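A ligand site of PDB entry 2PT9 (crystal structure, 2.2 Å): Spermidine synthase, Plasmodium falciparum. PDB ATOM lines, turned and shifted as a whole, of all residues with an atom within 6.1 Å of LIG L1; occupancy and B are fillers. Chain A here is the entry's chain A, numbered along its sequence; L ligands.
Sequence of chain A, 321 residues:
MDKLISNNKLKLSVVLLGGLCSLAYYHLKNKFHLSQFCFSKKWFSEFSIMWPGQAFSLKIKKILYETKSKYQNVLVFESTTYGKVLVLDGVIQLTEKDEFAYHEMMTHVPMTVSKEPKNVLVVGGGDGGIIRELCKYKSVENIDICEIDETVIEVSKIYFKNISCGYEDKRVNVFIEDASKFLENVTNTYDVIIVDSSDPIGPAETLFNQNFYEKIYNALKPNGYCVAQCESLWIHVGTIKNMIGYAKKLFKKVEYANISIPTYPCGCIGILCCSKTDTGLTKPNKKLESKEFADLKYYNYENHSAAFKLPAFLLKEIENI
OD2 of Asp 196 is in salt-bridge range of N1 of LIG L1 (2.7 Å). N of Ile 148 sits at hydrogen-bond distance from N5 of LIG L1 (3.2 Å). The side-chain carboxylate of Asp 127 is in salt-bridge range of a nitrogen (N1) of LIG L1 (2.7 Å). A nitrogen (N4) of LIG L1 lies within hydrogen-bond range of the side-chain carboxylate (OD1) of Asp 178 (2.6 Å). The side-chain amide nitrogen (NE2) of Gln 72 is in hydrogen-bond range of an oxygen (O2) of LIG L1. N of Ala 179 is in hydrogen-bond range of N6 of LIG L1, 3.1 Å away. A ring nitrogen (NE2) of His 103 is in hydrogen-bond range of a nitrogen (N1) of LIG L1 (2.6 Å). A nitrogen (N4) of LIG L1 sits at hydrogen-bond distance from the backbone carbonyl oxygen of Pro 203 (3.0 Å). The side-chain carboxylate (OE1) of Glu 147 is in hydrogen-bond range of an oxygen (O3) of LIG L1, 2.5 Å away. The backbone NH (N) of Ala 204 lies within hydrogen-bond range of a nitrogen (N3) of LIG L1, 3.3 Å away.
The backbone carbonyl oxygen (O) of Gln 93 lies within hydrogen-bond range of the side-chain hydroxyl (OH) of Tyr 264 (2.6 Å). OD1 of Asp 178 sits close to N of Ser 180 (3.3 Å). The backbone NH (N) of Gln 93 is in hydrogen-bond range of the backbone carbonyl oxygen (O) of Leu 86 (2.8 Å). The backbone NH (N) of Gly 124 is in hydrogen-bond range of the backbone carbonyl oxygen (O) of Cys 146, 2.8 Å away. The side-chain carboxylate (OE1) of Glu 147 is in hydrogen-bond range of the backbone NH (N) of Gly 126 (2.9 Å). The side-chain sulfur (SG) of Cys 146 lies within hydrogen-bond range of the backbone carbonyl oxygen (O) of Glu 177, 3.4 Å away. The side-chain carboxylate (OD1) of Asp 196 sits at hydrogen-bond distance from the side-chain hydroxyl (OH) of Tyr 102, 2.7 Å away. The side-chain carboxylate (OE2) of Glu 147 sits at hydrogen-bond distance from the backbone NH (N) of Asp 149 (2.9 Å).
Leu 88 touches LIG L1 (CD1 to C9, 3.8 Å). Gln 93 touches LIG L1 (NE2 to C3, 3.5 Å). Tyr 102 touches LIG L1 (CE2 to C1, 3.9 Å). Gly 124 touches LIG L1. Gly 125 touches LIG L1 (N to C6, 3.6 Å). Gly 126 touches LIG L1. O of Cys 146 touches C14 of LIG L1, at 3.6 Å. Asp 149 touches LIG L1 (CB to O2, 3.9 Å). Val 152 touches LIG L1 (CG1 to O3, 3.3 Å). Glu 177 touches LIG L1. Ser 197 touches LIG L1 (CA to O1, 3.7 Å). Ser 198 touches LIG L1. OG1 of Thr 206 touches N4 of LIG L1 (3.5 Å). Leu 207 touches LIG L1. Hydrophobic or aromatic side chains within 4 Å of LIG L1: Leu 88, Tyr 102, His 103, Ile 148, Val 152, Ala 179, Pro 203, Ala 204 and Leu 207. Within 4 Å of LIG L1: Gln 72, Leu 88, Gln 93, Tyr 102, His 103, Gly 124, Gly 125, Gly 126, Asp 127, Cys 146, Glu 147, Ile 148, Asp 149, Val 152, Glu 177, Asp 178, Ala 179, Asp 196, Ser 197, Ser 198, Pro 203, Ala 204, Thr 206 and Leu 207. The nearest printed residue that does not touch LIG L1 is Tyr 264 (4.05 Å).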
ATOM      1  N   GLN A  72     -15.263   4.277 -34.280  1.00  0.00           N
ATOM      2  CA  GLN A  72     -14.835   2.868 -34.236  1.00  0.00           C
ATOM      3  C   GLN A  72     -15.687   1.883 -35.025  1.00  0.00           C
ATOM      4  O   GLN A  72     -16.826   2.161 -35.379  1.00  0.00           O
ATOM      5  CB  GLN A  72     -14.683   2.387 -32.769  1.00  0.00           C
ATOM      6  CG  GLN A  72     -15.958   2.360 -31.928  1.00  0.00           C
ATOM      7  CD  GLN A  72     -15.711   2.695 -30.445  1.00  0.00           C
ATOM      8  OE1 GLN A  72     -14.690   2.310 -29.865  1.00  0.00           O
ATOM      9  NE2 GLN A  72     -16.646   3.408 -29.847  1.00  0.00           N
ATOM     10  N   LEU A  86     -20.112  -7.836 -27.585  1.00  0.00           N
ATOM     11  CA  LEU A  86     -19.867  -6.562 -28.173  1.00  0.00           C
ATOM     12  C   LEU A  86     -18.384  -6.447 -28.451  1.00  0.00           C
ATOM     13  O   LEU A  86     -17.555  -6.581 -27.554  1.00  0.00           O
ATOM     14  CB  LEU A  86     -20.350  -5.437 -27.240  1.00  0.00           C
ATOM     15  CG  LEU A  86     -20.021  -4.020 -27.704  1.00  0.00           C
ATOM     16  CD1 LEU A  86     -20.695  -3.744 -29.047  1.00  0.00           C
ATOM     17  CD2 LEU A  86     -20.491  -3.023 -26.653  1.00  0.00           C
ATOM     18  N   LEU A  88     -15.480  -3.918 -30.303  1.00  0.00           N
ATOM     19  CA  LEU A  88     -15.295  -2.552 -30.747  1.00  0.00           C
ATOM     20  C   LEU A  88     -13.888  -2.455 -31.255  1.00  0.00           C
ATOM     21  O   LEU A  88     -12.955  -2.694 -30.501  1.00  0.00           O
ATOM     22  CB  LEU A  88     -15.439  -1.600 -29.574  1.00  0.00           C
ATOM     23  CG  LEU A  88     -16.819  -1.228 -29.070  1.00  0.00           C
ATOM     24  CD1 LEU A  88     -16.722  -0.100 -28.035  1.00  0.00           C
ATOM     25  CD2 LEU A  88     -17.649  -0.769 -30.247  1.00  0.00           C
ATOM     26  N   GLN A  93     -15.309  -6.287 -25.857  1.00  0.00           N
ATOM     27  CA  GLN A  93     -15.573  -5.254 -24.844  1.00  0.00           C
ATOM     28  C   GLN A  93     -16.450  -5.831 -23.777  1.00  0.00           C
ATOM     29  O   GLN A  93     -16.349  -5.470 -22.606  1.00  0.00           O
ATOM     30  CB  GLN A  93     -16.299  -4.052 -25.459  1.00  0.00           C
ATOM     31  CG  GLN A  93     -15.511  -3.358 -26.539  1.00  0.00           C
ATOM     32  CD  GLN A  93     -14.289  -2.652 -25.999  1.00  0.00           C
ATOM     33  OE1 GLN A  93     -13.174  -2.874 -26.463  1.00  0.00           O
ATOM     34  NE2 GLN A  93     -14.492  -1.806 -24.988  1.00  0.00           N
ATOM     35  N   LEU A  94     -17.345  -6.722 -24.177  1.00  0.00           N
ATOM     36  CA  LEU A  94     -18.110  -7.454 -23.201  1.00  0.00           C
ATOM     37  C   LEU A  94     -18.838  -8.610 -23.812  1.00  0.00           C
ATOM     38  O   LEU A  94     -19.087  -8.618 -25.015  1.00  0.00           O
ATOM     39  CB  LEU A  94     -19.093  -6.534 -22.462  1.00  0.00           C
ATOM     40  CG  LEU A  94     -20.357  -5.896 -23.022  1.00  0.00           C
ATOM     41  CD1 LEU A  94     -21.347  -6.908 -23.530  1.00  0.00           C
ATOM     42  CD2 LEU A  94     -20.988  -5.135 -21.882  1.00  0.00           C
ATOM     43  N   TYR A 102     -16.660  -7.768 -14.152  1.00  0.00           N
ATOM     44  CA  TYR A 102     -16.042  -6.462 -14.328  1.00  0.00           C
ATOM     45  C   TYR A 102     -16.939  -5.306 -13.820  1.00  0.00           C
ATOM     46  O   TYR A 102     -16.472  -4.408 -13.146  1.00  0.00           O
ATOM     47  CB  TYR A 102     -15.741  -6.290 -15.802  1.00  0.00           C
ATOM     48  CG  TYR A 102     -15.186  -4.945 -16.189  1.00  0.00           C
ATOM     49  CD1 TYR A 102     -13.864  -4.617 -15.959  1.00  0.00           C
ATOM     50  CD2 TYR A 102     -15.995  -3.996 -16.813  1.00  0.00           C
ATOM     51  CE1 TYR A 102     -13.362  -3.379 -16.325  1.00  0.00           C
ATOM     52  CE2 TYR A 102     -15.531  -2.772 -17.166  1.00  0.00           C
ATOM     53  CZ  TYR A 102     -14.205  -2.464 -16.932  1.00  0.00           C
ATOM     54  OH  TYR A 102     -13.723  -1.235 -17.326  1.00  0.00           O
ATOM     55  N   HIS A 103     -18.227  -5.354 -14.128  1.00  0.00           N
ATOM     56  CA  HIS A 103     -19.110  -4.242 -13.744  1.00  0.00           C
ATOM     57  C   HIS A 103     -19.333  -4.130 -12.216  1.00  0.00           C
ATOM     58  O   HIS A 103     -19.327  -3.034 -11.665  1.00  0.00           O
ATOM     59  CB  HIS A 103     -20.429  -4.318 -14.516  1.00  0.00           C
ATOM     60  CG  HIS A 103     -20.282  -4.070 -15.996  1.00  0.00           C
ATOM     61  ND1 HIS A 103     -20.942  -4.828 -16.943  1.00  0.00           N
ATOM     62  CD2 HIS A 103     -19.535  -3.165 -16.671  1.00  0.00           C
ATOM     63  CE1 HIS A 103     -20.614  -4.390 -18.146  1.00  0.00           C
ATOM     64  NE2 HIS A 103     -19.756  -3.382 -18.004  1.00  0.00           N
ATOM     65  N   VAL A 123     -17.007   7.419 -16.960  1.00  0.00           N
ATOM     66  CA  VAL A 123     -16.330   7.831 -18.167  1.00  0.00           C
ATOM     67  C   VAL A 123     -16.260   6.629 -19.094  1.00  0.00           C
ATOM     68  O   VAL A 123     -15.815   5.567 -18.682  1.00  0.00           O
ATOM     69  CB  VAL A 123     -14.918   8.314 -17.856  1.00  0.00           C
ATOM     70  CG1 VAL A 123     -14.068   8.392 -19.117  1.00  0.00           C
ATOM     71  CG2 VAL A 123     -14.962   9.641 -17.097  1.00  0.00           C
ATOM     72  N   GLY A 124     -16.689   6.786 -20.352  1.00  0.00           N
ATOM     73  CA  GLY A 124     -16.861   5.647 -21.231  1.00  0.00           C
ATOM     74  C   GLY A 124     -18.093   4.891 -20.750  1.00  0.00           C
ATOM     75  O   GLY A 124     -19.087   5.489 -20.363  1.00  0.00           O
ATOM     76  N   GLY A 125     -18.026   3.565 -20.764  1.00  0.00           N
ATOM     77  CA  GLY A 125     -19.112   2.725 -20.256  1.00  0.00           C
ATOM     78  C   GLY A 125     -20.437   2.885 -20.984  1.00  0.00           C
ATOM     79  O   GLY A 125     -21.490   2.884 -20.342  1.00  0.00           O
ATOM     80  N   GLY A 126     -20.386   3.001 -22.325  1.00  0.00           N
ATOM     81  CA  GLY A 126     -21.549   3.206 -23.164  1.00  0.00           C
ATOM     82  C   GLY A 126     -22.631   2.133 -23.037  1.00  0.00           C
ATOM     83  O   GLY A 126     -23.808   2.451 -23.114  1.00  0.00           O
ATOM     84  N   ASP A 127     -22.205   0.890 -22.833  1.00  0.00           N
ATOM     85  CA  ASP A 127     -23.088  -0.289 -22.684  1.00  0.00           C
ATOM     86  C   ASP A 127     -24.069  -0.253 -21.518  1.00  0.00           C
ATOM     87  O   ASP A 127     -25.105  -0.946 -21.541  1.00  0.00           O
ATOM     88  CB  ASP A 127     -22.244  -1.561 -22.555  1.00  0.00           C
ATOM     89  CG  ASP A 127     -21.327  -1.542 -21.333  1.00  0.00           C
ATOM     90  OD1 ASP A 127     -21.654  -2.219 -20.337  1.00  0.00           O
ATOM     91  OD2 ASP A 127     -20.276  -0.826 -21.357  1.00  0.00           O
ATOM     92  N   GLY A 128     -23.721   0.505 -20.469  1.00  0.00           N
ATOM     93  CA  GLY A 128     -24.602   0.730 -19.321  1.00  0.00           C
ATOM     94  C   GLY A 128     -24.408  -0.193 -18.132  1.00  0.00           C
ATOM     95  O   GLY A 128     -25.142  -0.095 -17.162  1.00  0.00           O
ATOM     96  N   GLY A 129     -23.419  -1.075 -18.185  1.00  0.00           N
ATOM     97  CA  GLY A 129     -23.200  -2.049 -17.107  1.00  0.00           C
ATOM     98  C   GLY A 129     -22.905  -1.405 -15.769  1.00  0.00           C
ATOM     99  O   GLY A 129     -23.493  -1.780 -14.753  1.00  0.00           O
ATOM    100  N   ILE A 130     -22.008  -0.419 -15.766  1.00  0.00           N
ATOM    101  CA  ILE A 130     -21.711   0.314 -14.548  1.00  0.00           C
ATOM    102  C   ILE A 130     -22.958   1.010 -13.987  1.00  0.00           C
ATOM    103  O   ILE A 130     -23.245   0.890 -12.779  1.00  0.00           O
ATOM    104  CB  ILE A 130     -20.597   1.368 -14.743  1.00  0.00           C
ATOM    105  CG1 ILE A 130     -19.312   0.752 -15.299  1.00  0.00           C
ATOM    106  CG2 ILE A 130     -20.366   2.083 -13.460  1.00  0.00           C
ATOM    107  CD1 ILE A 130     -18.752  -0.456 -14.530  1.00  0.00           C
ATOM    108  N   CYS A 146     -20.283  10.022 -19.436  1.00  0.00           N
ATOM    109  CA  CYS A 146     -19.679  10.722 -20.539  1.00  0.00           C
ATOM    110  C   CYS A 146     -19.049   9.692 -21.480  1.00  0.00           C
ATOM    111  O   CYS A 146     -18.043   9.096 -21.163  1.00  0.00           O
ATOM    112  CB  CYS A 146     -18.621  11.689 -20.052  1.00  0.00           C
ATOM    113  SG  CYS A 146     -17.947  12.593 -21.431  1.00  0.00           S
ATOM    114  N   GLU A 147     -19.700   9.485 -22.623  1.00  0.00           N
ATOM    115  CA  GLU A 147     -19.352   8.437 -23.571  1.00  0.00           C
ATOM    116  C   GLU A 147     -19.208   9.112 -24.934  1.00  0.00           C
ATOM    117  O   GLU A 147     -20.106   9.840 -25.350  1.00  0.00           O
ATOM    118  CB  GLU A 147     -20.468   7.367 -23.557  1.00  0.00           C
ATOM    119  CG  GLU A 147     -20.624   6.503 -24.819  1.00  0.00           C
ATOM    120  CD  GLU A 147     -19.449   5.616 -25.096  1.00  0.00           C
ATOM    121  OE1 GLU A 147     -19.128   4.780 -24.240  1.00  0.00           O
ATOM    122  OE2 GLU A 147     -18.825   5.746 -26.173  1.00  0.00           O
ATOM    123  N   ILE A 148     -18.073   8.913 -25.607  1.00  0.00           N
ATOM    124  CA  ILE A 148     -17.760   9.629 -26.856  1.00  0.00           C
ATOM    125  C   ILE A 148     -18.649   9.247 -28.054  1.00  0.00           C
ATOM    126  O   ILE A 148     -18.911  10.086 -28.941  1.00  0.00           O
ATOM    127  CB  ILE A 148     -16.251   9.490 -27.234  1.00  0.00           C
ATOM    128  CG1 ILE A 148     -15.814  10.645 -28.155  1.00  0.00           C
ATOM    129  CG2 ILE A 148     -15.959   8.105 -27.818  1.00  0.00           C
ATOM    130  CD1 ILE A 148     -14.326  10.733 -28.365  1.00  0.00           C
ATOM    131  N   ASP A 149     -19.150   8.002 -28.024  1.00  0.00           N
ATOM    132  CA  ASP A 149     -19.748   7.330 -29.153  1.00  0.00           C
ATOM    133  C   ASP A 149     -21.194   6.858 -28.884  1.00  0.00           C
ATOM    134  O   ASP A 149     -21.418   5.851 -28.218  1.00  0.00           O
ATOM    135  CB  ASP A 149     -18.855   6.152 -29.564  1.00  0.00           C
ATOM    136  CG  ASP A 149     -19.202   5.576 -30.936  1.00  0.00           C
ATOM    137  OD1 ASP A 149     -20.301   5.885 -31.470  1.00  0.00           O
ATOM    138  OD2 ASP A 149     -18.386   4.794 -31.470  1.00  0.00           O
ATOM    139  N   VAL A 152     -22.561   3.208 -29.546  1.00  0.00           N
ATOM    140  CA  VAL A 152     -22.361   2.214 -28.505  1.00  0.00           C
ATOM    141  C   VAL A 152     -23.589   2.159 -27.586  1.00  0.00           C
ATOM    142  O   VAL A 152     -24.141   1.079 -27.365  1.00  0.00           O
ATOM    143  CB  VAL A 152     -21.062   2.491 -27.693  1.00  0.00           C
ATOM    144  CG1 VAL A 152     -20.867   1.409 -26.623  1.00  0.00           C
ATOM    145  CG2 VAL A 152     -19.827   2.569 -28.606  1.00  0.00           C
ATOM    146  N   GLU A 177     -19.571  12.990 -25.648  1.00  0.00           N
ATOM    147  CA  GLU A 177     -18.426  13.881 -25.656  1.00  0.00           C
ATOM    148  C   GLU A 177     -17.179  13.112 -25.314  1.00  0.00           C
ATOM    149  O   GLU A 177     -17.266  12.061 -24.670  1.00  0.00           O
ATOM    150  CB  GLU A 177     -18.640  14.938 -24.566  1.00  0.00           C
ATOM    151  CG  GLU A 177     -17.826  16.222 -24.757  1.00  0.00           C
ATOM    152  CD  GLU A 177     -18.219  17.306 -23.745  1.00  0.00           C
ATOM    153  OE1 GLU A 177     -19.402  17.320 -23.279  1.00  0.00           O
ATOM    154  OE2 GLU A 177     -17.351  18.153 -23.438  1.00  0.00           O
ATOM    155  N   ASP A 178     -16.028  13.629 -25.735  1.00  0.00           N
ATOM    156  CA  ASP A 178     -14.761  13.070 -25.293  1.00  0.00           C
ATOM    157  C   ASP A 178     -14.596  13.412 -23.811  1.00  0.00           C
ATOM    158  O   ASP A 178     -14.560  14.596 -23.462  1.00  0.00           O
ATOM    159  CB  ASP A 178     -13.596  13.678 -26.090  1.00  0.00           C
ATOM    160  CG  ASP A 178     -12.275  13.008 -25.778  1.00  0.00           C
ATOM    161  OD1 ASP A 178     -12.228  12.043 -24.978  1.00  0.00           O
ATOM    162  OD2 ASP A 178     -11.246  13.436 -26.334  1.00  0.00           O
ATOM    163  N   ALA A 179     -14.519  12.392 -22.948  1.00  0.00           N
ATOM    164  CA  ALA A 179     -14.349  12.635 -21.497  1.00  0.00           C
ATOM    165  C   ALA A 179     -13.219  13.611 -21.227  1.00  0.00           C
ATOM    166  O   ALA A 179     -13.320  14.429 -20.333  1.00  0.00           O
ATOM    167  CB  ALA A 179     -14.115  11.369 -20.748  1.00  0.00           C
ATOM    168  N   SER A 180     -12.148  13.534 -22.006  1.00  0.00           N
ATOM    169  CA  SER A 180     -11.039  14.478 -21.923  1.00  0.00           C
ATOM    170  C   SER A 180     -11.487  15.948 -22.011  1.00  0.00           C
ATOM    171  O   SER A 180     -11.006  16.779 -21.221  1.00  0.00           O
ATOM    172  CB  SER A 180     -10.029  14.153 -23.009  1.00  0.00           C
ATOM    173  OG  SER A 180      -9.083  15.196 -23.120  1.00  0.00           O
ATOM    174  N   ASP A 196     -14.340   3.568 -17.260  1.00  0.00           N
ATOM    175  CA  ASP A 196     -14.621   2.283 -17.854  1.00  0.00           C
ATOM    176  C   ASP A 196     -14.394   2.409 -19.340  1.00  0.00           C
ATOM    177  O   ASP A 196     -15.319   2.268 -20.139  1.00  0.00           O
ATOM    178  CB  ASP A 196     -16.060   1.899 -17.563  1.00  0.00           C
ATOM    179  CG  ASP A 196     -16.515   0.655 -18.319  1.00  0.00           C
ATOM    180  OD1 ASP A 196     -15.668  -0.123 -18.812  1.00  0.00           O
ATOM    181  OD2 ASP A 196     -17.736   0.474 -18.426  1.00  0.00           O
ATOM    182  N   SER A 197     -13.151   2.736 -19.702  1.00  0.00           N
ATOM    183  CA  SER A 197     -12.731   2.946 -21.082  1.00  0.00           C
ATOM    184  C   SER A 197     -12.335   1.641 -21.814  1.00  0.00           C
ATOM    185  O   SER A 197     -12.081   0.610 -21.194  1.00  0.00           O
ATOM    186  CB  SER A 197     -11.528   3.853 -21.103  1.00  0.00           C
ATOM    187  OG  SER A 197     -10.398   3.152 -20.591  1.00  0.00           O
ATOM    188  N   SER A 198     -12.259   1.735 -23.130  1.00  0.00           N
ATOM    189  CA  SER A 198     -11.610   0.728 -23.974  1.00  0.00           C
ATOM    190  C   SER A 198     -10.056   0.897 -23.946  1.00  0.00           C
ATOM    191  O   SER A 198      -9.526   1.624 -23.094  1.00  0.00           O
ATOM    192  CB  SER A 198     -12.179   0.837 -25.406  1.00  0.00           C
ATOM    193  OG  SER A 198     -12.038   2.146 -25.939  1.00  0.00           O
ATOM    194  N   GLY A 202      -7.135   4.032 -30.262  1.00  0.00           N
ATOM    195  CA  GLY A 202      -8.439   4.502 -30.706  1.00  0.00           C
ATOM    196  C   GLY A 202      -8.861   5.722 -29.916  1.00  0.00           C
ATOM    197  O   GLY A 202      -8.029   6.551 -29.564  1.00  0.00           O
ATOM    198  N   PRO A 203     -10.171   5.809 -29.598  1.00  0.00           N
ATOM    199  CA  PRO A 203     -10.759   6.968 -28.917  1.00  0.00           C
ATOM    200  C   PRO A 203     -10.298   7.168 -27.457  1.00  0.00           C
ATOM    201  O   PRO A 203     -10.319   8.290 -26.963  1.00  0.00           O
ATOM    202  CB  PRO A 203     -12.269   6.709 -28.968  1.00  0.00           C
ATOM    203  CG  PRO A 203     -12.462   5.465 -29.785  1.00  0.00           C
ATOM    204  CD  PRO A 203     -11.159   4.760 -29.884  1.00  0.00           C
ATOM    205  N   ALA A 204      -9.892   6.078 -26.795  1.00  0.00           N
ATOM    206  CA  ALA A 204      -9.495   6.093 -25.378  1.00  0.00           C
ATOM    207  C   ALA A 204      -8.047   6.515 -25.188  1.00  0.00           C
ATOM    208  O   ALA A 204      -7.541   6.549 -24.071  1.00  0.00           O
ATOM    209  CB  ALA A 204      -9.746   4.736 -24.733  1.00  0.00           C
ATOM    210  N   GLU A 205      -7.415   6.845 -26.306  1.00  0.00           N
ATOM    211  CA  GLU A 205      -6.029   7.293 -26.346  1.00  0.00           C
ATOM    212  C   GLU A 205      -5.807   8.557 -25.502  1.00  0.00           C
ATOM    213  O   GLU A 205      -4.749   8.715 -24.880  1.00  0.00           O
ATOM    214  CB  GLU A 205      -5.681   7.557 -27.808  1.00  0.00           C
ATOM    215  CG  GLU A 205      -4.297   8.099 -28.092  1.00  0.00           C
ATOM    216  CD  GLU A 205      -4.227   8.724 -29.486  1.00  0.00           C
ATOM    217  OE1 GLU A 205      -3.100   8.852 -30.021  1.00  0.00           O
ATOM    218  OE2 GLU A 205      -5.295   9.086 -30.041  1.00  0.00           O
ATOM    219  N   THR A 206      -6.798   9.441 -25.491  1.00  0.00           N
ATOM    220  CA  THR A 206      -6.759  10.688 -24.736  1.00  0.00           C
ATOM    221  C   THR A 206      -6.886  10.515 -23.210  1.00  0.00           C
ATOM    222  O   THR A 206      -6.689  11.467 -22.456  1.00  0.00           O
ATOM    223  CB  THR A 206      -7.841  11.671 -25.224  1.00  0.00           C
ATOM    224  OG1 THR A 206      -9.142  11.100 -24.996  1.00  0.00           O
ATOM    225  CG2 THR A 206      -7.671  11.964 -26.703  1.00  0.00           C
ATOM    226  N   LEU A 207      -7.185   9.297 -22.756  1.00  0.00           N
ATOM    227  CA  LEU A 207      -7.400   9.016 -21.331  1.00  0.00           C
ATOM    228  C   LEU A 207      -6.199   8.354 -20.633  1.00  0.00           C
ATOM    229  O   LEU A 207      -6.207   8.138 -19.414  1.00  0.00           O
ATOM    230  CB  LEU A 207      -8.652   8.135 -21.141  1.00  0.00           C
ATOM    231  CG  LEU A 207      -9.923   8.388 -21.960  1.00  0.00           C
ATOM    232  CD1 LEU A 207     -10.938   7.309 -21.668  1.00  0.00           C
ATOM    233  CD2 LEU A 207     -10.522   9.783 -21.736  1.00  0.00           C
ATOM    234  N   TYR A 264     -11.388 -11.314 -21.505  1.00  0.00           N
ATOM    235  CA  TYR A 264     -10.393 -10.283 -21.716  1.00  0.00           C
ATOM    236  C   TYR A 264      -9.013 -10.956 -21.821  1.00  0.00           C
ATOM    237  O   TYR A 264      -8.804 -12.037 -21.263  1.00  0.00           O
ATOM    238  CB  TYR A 264     -10.436  -9.268 -20.566  1.00  0.00           C
ATOM    239  CG  TYR A 264     -11.668  -8.387 -20.523  1.00  0.00           C
ATOM    240  CD1 TYR A 264     -12.400  -8.095 -21.686  1.00  0.00           C
ATOM    241  CD2 TYR A 264     -12.070  -7.785 -19.330  1.00  0.00           C
ATOM    242  CE1 TYR A 264     -13.504  -7.257 -21.655  1.00  0.00           C
ATOM    243  CE2 TYR A 264     -13.176  -6.933 -19.281  1.00  0.00           C
ATOM    244  CZ  TYR A 264     -13.901  -6.682 -20.446  1.00  0.00           C
ATOM    245  OH  TYR A 264     -15.005  -5.840 -20.395  1.00  0.00           O
HETATM  246  C1  LIG L   1     -17.733  -2.821 -20.425  1.00  0.00           C
HETATM  247  N1  LIG L   1     -18.468  -1.802 -19.654  1.00  0.00           N
HETATM  248  C2  LIG L   1     -16.542  -2.167 -21.119  1.00  0.00           C
HETATM  249  C3  LIG L   1     -16.921  -1.711 -22.519  1.00  0.00           C
HETATM  250  S1  LIG L   1     -17.454   0.025 -22.651  1.00  0.00           S
HETATM  251  C4  LIG L   1     -18.598  -0.243 -23.996  1.00  0.00           C
HETATM  252  C5  LIG L   1     -16.063   1.006 -23.423  1.00  0.00           C
HETATM  253  C6  LIG L   1     -16.371   2.490 -23.809  1.00  0.00           C
HETATM  254  O1  LIG L   1     -15.291   3.485 -23.757  1.00  0.00           O
HETATM  255  C7  LIG L   1     -15.766   4.523 -24.613  1.00  0.00           C
HETATM  256  C8  LIG L   1     -15.969   3.696 -25.863  1.00  0.00           C
HETATM  257  O2  LIG L   1     -16.752   4.427 -26.809  1.00  0.00           O
HETATM  258  C9  LIG L   1     -16.743   2.496 -25.291  1.00  0.00           C
HETATM  259  O3  LIG L   1     -18.123   2.750 -25.364  1.00  0.00           O
HETATM  260  N2  LIG L   1     -14.730   5.547 -24.842  1.00  0.00           N
HETATM  261  C10 LIG L   1     -13.560   5.328 -25.440  1.00  0.00           C
HETATM  262  N3  LIG L   1     -12.860   6.473 -25.459  1.00  0.00           N
HETATM  263  C11 LIG L   1     -13.582   7.436 -24.871  1.00  0.00           C
HETATM  264  C12 LIG L   1     -13.352   8.790 -24.608  1.00  0.00           C
HETATM  265  N4  LIG L   1     -12.214   9.400 -24.967  1.00  0.00           N
HETATM  266  C13 LIG L   1     -14.782   6.844 -24.476  1.00  0.00           C
HETATM  267  N5  LIG L   1     -15.694   7.610 -23.837  1.00  0.00           N
HETATM  268  C14 LIG L   1     -15.456   8.908 -23.603  1.00  0.00           C
HETATM  269  N6  LIG L   1     -14.317   9.504 -23.979  1.00  0.00           N
HETATM  270  N1  LG2 L   2      -8.872  -5.268 -23.794  1.00  0.00           N
HETATM  271  C1  LG2 L   2      -9.693  -4.452 -22.941  1.00  0.00           C
HETATM  272  C2  LG2 L   2     -10.351  -5.334 -21.873  1.00  0.00           C
HETATM  273  C3  LG2 L   2     -10.782  -3.755 -23.759  1.00  0.00           C
HETATM  274  C4  LG2 L   2     -12.083  -3.513 -22.993  1.00  0.00           C
HETATM  275  C5  LG2 L   2     -11.838  -3.289 -21.497  1.00  0.00           C
HETATM  276  C6  LG2 L   2     -13.156  -3.006 -20.770  1.00  0.00           C
HETATM  277  C7  LG2 L   2     -11.151  -4.496 -20.871  1.00  0.00           C
